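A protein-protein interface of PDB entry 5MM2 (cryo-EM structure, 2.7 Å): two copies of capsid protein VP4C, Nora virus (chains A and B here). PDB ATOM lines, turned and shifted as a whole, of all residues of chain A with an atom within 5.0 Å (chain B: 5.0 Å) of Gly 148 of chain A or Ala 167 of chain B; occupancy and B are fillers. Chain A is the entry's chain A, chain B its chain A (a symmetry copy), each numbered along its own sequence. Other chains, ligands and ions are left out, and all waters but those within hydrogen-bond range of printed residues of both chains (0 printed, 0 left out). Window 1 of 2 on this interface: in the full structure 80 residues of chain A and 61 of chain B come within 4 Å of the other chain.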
ATOM      1  N   PHE A  16     -17.031  34.701   3.319  1.00  0.00           N
ATOM      2  CA  PHE A  16     -17.949  34.272   2.278  1.00  0.00           C
ATOM      3  C   PHE A  16     -18.219  35.420   1.323  1.00  0.00           C
ATOM      4  O   PHE A  16     -18.336  36.570   1.742  1.00  0.00           O
ATOM      5  CB  PHE A  16     -19.248  33.775   2.888  1.00  0.00           C
ATOM      6  CG  PHE A  16     -19.051  32.703   3.901  1.00  0.00           C
ATOM      7  CD1 PHE A  16     -18.695  31.429   3.521  1.00  0.00           C
ATOM      8  CD2 PHE A  16     -19.236  32.966   5.240  1.00  0.00           C
ATOM      9  CE1 PHE A  16     -18.511  30.447   4.460  1.00  0.00           C
ATOM     10  CE2 PHE A  16     -19.050  31.992   6.174  1.00  0.00           C
ATOM     11  CZ  PHE A  16     -18.687  30.731   5.785  1.00  0.00           C
ATOM     12  N   THR A  18     -20.770  34.959  -1.129  1.00  0.00           N
ATOM     13  CA  THR A  18     -22.183  34.796  -1.414  1.00  0.00           C
ATOM     14  C   THR A  18     -22.920  34.663  -0.091  1.00  0.00           C
ATOM     15  O   THR A  18     -22.292  34.443   0.947  1.00  0.00           O
ATOM     16  CB  THR A  18     -22.428  33.554  -2.284  1.00  0.00           C
ATOM     17  OG1 THR A  18     -21.962  32.392  -1.598  1.00  0.00           O
ATOM     18  CG2 THR A  18     -21.722  33.679  -3.607  1.00  0.00           C
ATOM     19  N   PRO A  19     -24.243  34.823  -0.069  1.00  0.00           N
ATOM     20  CA  PRO A  19     -24.995  34.408   1.114  1.00  0.00           C
ATOM     21  C   PRO A  19     -24.982  32.896   1.267  1.00  0.00           C
ATOM     22  O   PRO A  19     -24.631  32.152   0.351  1.00  0.00           O
ATOM     23  CB  PRO A  19     -26.403  34.934   0.845  1.00  0.00           C
ATOM     24  CG  PRO A  19     -26.475  35.112  -0.594  1.00  0.00           C
ATOM     25  CD  PRO A  19     -25.118  35.540  -1.011  1.00  0.00           C
ATOM     26  N   THR A  21     -26.283  29.081   1.603  1.00  0.00           N
ATOM     27  CA  THR A  21     -27.233  28.357   0.768  1.00  0.00           C
ATOM     28  C   THR A  21     -28.552  28.141   1.495  1.00  0.00           C
ATOM     29  O   THR A  21     -29.622  28.299   0.898  1.00  0.00           O
ATOM     30  CB  THR A  21     -26.632  27.030   0.320  1.00  0.00           C
ATOM     31  OG1 THR A  21     -26.326  26.235   1.468  1.00  0.00           O
ATOM     32  CG2 THR A  21     -25.364  27.270  -0.443  1.00  0.00           C
ATOM     33  N   PHE A  99     -28.339  22.611  -0.558  1.00  0.00           N
ATOM     34  CA  PHE A  99     -28.825  22.220  -1.874  1.00  0.00           C
ATOM     35  C   PHE A  99     -29.695  20.978  -1.797  1.00  0.00           C
ATOM     36  O   PHE A  99     -30.837  20.974  -2.261  1.00  0.00           O
ATOM     37  CB  PHE A  99     -27.655  21.963  -2.813  1.00  0.00           C
ATOM     38  CG  PHE A  99     -26.955  23.190  -3.264  1.00  0.00           C
ATOM     39  CD1 PHE A  99     -27.484  23.956  -4.275  1.00  0.00           C
ATOM     40  CD2 PHE A  99     -25.753  23.560  -2.707  1.00  0.00           C
ATOM     41  CE1 PHE A  99     -26.835  25.076  -4.715  1.00  0.00           C
ATOM     42  CE2 PHE A  99     -25.103  24.685  -3.140  1.00  0.00           C
ATOM     43  CZ  PHE A  99     -25.650  25.445  -4.145  1.00  0.00           C
ATOM     44  N   HIS A 122     -15.460  28.288  -8.057  1.00  0.00           N
ATOM     45  CA  HIS A 122     -15.999  26.945  -8.168  1.00  0.00           C
ATOM     46  C   HIS A 122     -17.314  26.822  -7.417  1.00  0.00           C
ATOM     47  O   HIS A 122     -17.534  27.469  -6.395  1.00  0.00           O
ATOM     48  CB  HIS A 122     -15.013  25.898  -7.671  1.00  0.00           C
ATOM     49  CG  HIS A 122     -14.686  26.015  -6.223  1.00  0.00           C
ATOM     50  ND1 HIS A 122     -13.803  26.950  -5.739  1.00  0.00           N
ATOM     51  CD2 HIS A 122     -15.086  25.287  -5.157  1.00  0.00           C
ATOM     52  CE1 HIS A 122     -13.700  26.817  -4.431  1.00  0.00           C
ATOM     53  NE2 HIS A 122     -14.464  25.812  -4.053  1.00  0.00           N
ATOM     54  N   ASN A 123     -18.189  25.981  -7.957  1.00  0.00           N
ATOM     55  CA  ASN A 123     -19.490  25.700  -7.378  1.00  0.00           C
ATOM     56  C   ASN A 123     -19.953  24.371  -7.947  1.00  0.00           C
ATOM     57  O   ASN A 123     -19.553  23.994  -9.046  1.00  0.00           O
ATOM     58  CB  ASN A 123     -20.487  26.812  -7.701  1.00  0.00           C
ATOM     59  CG  ASN A 123     -21.721  26.759  -6.840  1.00  0.00           C
ATOM     60  OD1 ASN A 123     -21.843  25.911  -5.968  1.00  0.00           O
ATOM     61  ND2 ASN A 123     -22.641  27.676  -7.076  1.00  0.00           N
ATOM     62  N   VAL A 146     -24.845  33.105  -7.934  1.00  0.00           N
ATOM     63  CA  VAL A 146     -25.602  32.006  -7.355  1.00  0.00           C
ATOM     64  C   VAL A 146     -24.980  31.664  -6.008  1.00  0.00           C
ATOM     65  O   VAL A 146     -23.768  31.811  -5.827  1.00  0.00           O
ATOM     66  CB  VAL A 146     -25.634  30.807  -8.329  1.00  0.00           C
ATOM     67  CG1 VAL A 146     -24.246  30.320  -8.655  1.00  0.00           C
ATOM     68  CG2 VAL A 146     -26.496  29.671  -7.815  1.00  0.00           C
ATOM     69  N   ALA A 147     -25.816  31.297  -5.041  1.00  0.00           N
ATOM     70  CA  ALA A 147     -25.334  31.029  -3.698  1.00  0.00           C
ATOM     71  C   ALA A 147     -24.483  29.767  -3.672  1.00  0.00           C
ATOM     72  O   ALA A 147     -24.768  28.794  -4.370  1.00  0.00           O
ATOM     73  CB  ALA A 147     -26.500  30.890  -2.728  1.00  0.00           C
ATOM     74  N   GLY A 148     -23.429  29.795  -2.868  1.00  0.00           N
ATOM     75  CA  GLY A 148     -22.539  28.668  -2.722  1.00  0.00           C
ATOM     76  C   GLY A 148     -21.219  28.778  -3.445  1.00  0.00           C
ATOM     77  O   GLY A 148     -20.402  27.862  -3.340  1.00  0.00           O
ATOM     78  N   THR A 149     -20.982  29.862  -4.170  1.00  0.00           N
ATOM     79  CA  THR A 149     -19.755  30.036  -4.927  1.00  0.00           C
ATOM     80  C   THR A 149     -18.622  30.465  -4.009  1.00  0.00           C
ATOM     81  O   THR A 149     -18.787  31.368  -3.190  1.00  0.00           O
ATOM     82  CB  THR A 149     -19.972  31.079  -6.017  1.00  0.00           C
ATOM     83  OG1 THR A 149     -21.004  30.631  -6.896  1.00  0.00           O
ATOM     84  CG2 THR A 149     -18.725  31.319  -6.825  1.00  0.00           C
ATOM     85  N   ALA A 150     -17.474  29.815  -4.138  1.00  0.00           N
ATOM     86  CA  ALA A 150     -16.288  30.213  -3.408  1.00  0.00           C
ATOM     87  C   ALA A 150     -15.235  30.735  -4.370  1.00  0.00           C
ATOM     88  O   ALA A 150     -15.250  30.439  -5.563  1.00  0.00           O
ATOM     89  CB  ALA A 150     -15.728  29.047  -2.599  1.00  0.00           C
ATOM     90  N   SER A 213     -12.253  23.267  -1.974  1.00  0.00           N
ATOM     91  CA  SER A 213     -13.115  22.108  -1.888  1.00  0.00           C
ATOM     92  C   SER A 213     -14.551  22.531  -1.666  1.00  0.00           C
ATOM     93  O   SER A 213     -14.826  23.609  -1.140  1.00  0.00           O
ATOM     94  CB  SER A 213     -12.660  21.193  -0.758  1.00  0.00           C
ATOM     95  OG  SER A 213     -13.489  20.057  -0.679  1.00  0.00           O
ATOM     96  N   THR B 165     -13.432  32.163  -0.565  1.00  0.00           N
ATOM     97  CA  THR B 165     -14.825  32.112  -0.147  1.00  0.00           C
ATOM     98  C   THR B 165     -15.156  30.893   0.698  1.00  0.00           C
ATOM     99  O   THR B 165     -15.754  31.054   1.767  1.00  0.00           O
ATOM    100  CB  THR B 165     -15.731  32.160  -1.377  1.00  0.00           C
ATOM    101  OG1 THR B 165     -15.482  33.372  -2.090  1.00  0.00           O
ATOM    102  CG2 THR B 165     -17.197  32.119  -0.975  1.00  0.00           C
ATOM    103  N   ALA B 166     -14.790  29.688   0.235  1.00  0.00           N
ATOM    104  CA  ALA B 166     -15.046  28.421   0.922  1.00  0.00           C
ATOM    105  C   ALA B 166     -16.532  28.170   1.146  1.00  0.00           C
ATOM    106  O   ALA B 166     -17.040  28.412   2.242  1.00  0.00           O
ATOM    107  CB  ALA B 166     -14.271  28.320   2.240  1.00  0.00           C
ATOM    108  N   ALA B 167     -17.230  27.733   0.089  1.00  0.00           N
ATOM    109  CA  ALA B 167     -18.665  27.640  -0.194  1.00  0.00           C
ATOM    110  C   ALA B 167     -19.592  27.346   0.978  1.00  0.00           C
ATOM    111  O   ALA B 167     -19.284  26.508   1.831  1.00  0.00           O
ATOM    112  CB  ALA B 167     -18.886  26.554  -1.247  1.00  0.00           C
ATOM    113  N   PRO B 168     -20.814  28.054   1.043  1.00  0.00           N
ATOM    114  CA  PRO B 168     -21.687  28.009   2.228  1.00  0.00           C
ATOM    115  C   PRO B 168     -22.634  26.817   2.223  1.00  0.00           C
ATOM    116  O   PRO B 168     -23.854  26.954   2.190  1.00  0.00           O
ATOM    117  CB  PRO B 168     -22.436  29.339   2.125  1.00  0.00           C
ATOM    118  CG  PRO B 168     -22.530  29.577   0.684  1.00  0.00           C
ATOM    119  CD  PRO B 168     -21.286  29.043   0.064  1.00  0.00           C
ATOM    120  N   ILE B 169     -22.080  25.649   2.260  1.00  0.00           N
ATOM    121  CA  ILE B 169     -22.869  24.429   2.306  1.00  0.00           C
ATOM    122  C   ILE B 169     -22.935  23.938   3.742  1.00  0.00           C
ATOM    123  O   ILE B 169     -22.056  24.218   4.559  1.00  0.00           O
ATOM    124  CB  ILE B 169     -22.278  23.371   1.357  1.00  0.00           C
ATOM    125  CG1 ILE B 169     -20.832  23.075   1.731  1.00  0.00           C
ATOM    126  CG2 ILE B 169     -22.369  23.853  -0.069  1.00  0.00           C
ATOM    127  CD1 ILE B 169     -20.229  21.956   0.961  1.00  0.00           C
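Hydrophobic or aromatic side chains of chain A that line the printed part of chain B: Phe 16 and Ala 150.
Hydrophobic or aromatic side chains of chain B that line the printed part of chain A: Ala 167 and Pro 168.
Among the printed residues, 12 pairs touch across the chains.
Among the printed residues, no Asp or Glu carboxylate lies within 4 Å of a Lys or Arg side-chain nitrogen of the other chain.
No position is printed for both chains.
Of the 12 pairs that touch across the chains among the printed residues, none has its exchanged pair printed and touching as well.
N of Gly 148 of chain A is in hydrogen-bond range of OG1 of Thr 18 of chain A (3.2 Å).
The backbone NH of Ala 150 of chain A sits at hydrogen-bond distance from the backbone carbonyl oxygen of His 122 of chain A, at 3.3 Å.
The backbone carbonyl oxygen (O) of Val 146 of chain A is in hydrogen-bond range of the side-chain hydroxyl (OG1) of Thr 149 of chain A (3.2 Å).
The side-chain amide nitrogen of Asn 123 of chain A lies within hydrogen-bond range of the side-chain hydroxyl of Thr 149 of chain A (3.4 Å).
Gly 148 of chain A touches just these residues of chain B: Ala 167 and Pro 168.
Ala 167 of chain B touches two residues of chain A.
Of the printed residues of chain A, Thr 165 of chain B touches Phe 16 (3.4 Å), Thr 149 (2.8 Å) and Ala 150 (2.9 Å).
Printed residues of chain B within 4 Å of Ala 150 of chain A: Thr 165, Ala 166 and Ala 167.
Of the printed residues of chain B, Thr 18 of chain A touches Pro 168.
Of the printed residues of chain B, Thr 21 of chain A touches Pro 168 (2.7 Å) and Ile 169 (3.99 Å).
Of the printed residues of chain B, Pro 19 of chain A touches Pro 168.
Ser 213 of chain A touches none of the printed residues of chain B.
Phe 16 of chain A touches Thr 165 of chain B (CD1 to O, 3.4 Å).
Pro 168 of chain B touches Thr 18 of chain A.
Pro 168 of chain B touches Pro 19 of chain A.
Ile 169 of chain B touches Thr 21 of chain A.
Ala 167 of chain B touches Gly 148 of chain A.
Pro 168 of chain B touches Gly 148 of chain A (CD to CA, 3.1 Å).
Thr 149 of chain A touches Thr 165 of chain B (O to CG2, 2.8 Å).
Ala 150 of chain A touches Thr 165 of chain B.
Ala 150 of chain A touches Ala 166 of chain B.
Ala 150 of chain A touches Ala 167 of chain B.
The backbone carbonyl oxygen of Pro 168 of chain B is in hydrogen-bond range of the side-chain hydroxyl of Thr 21 of chain A, 2.7 Å away.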
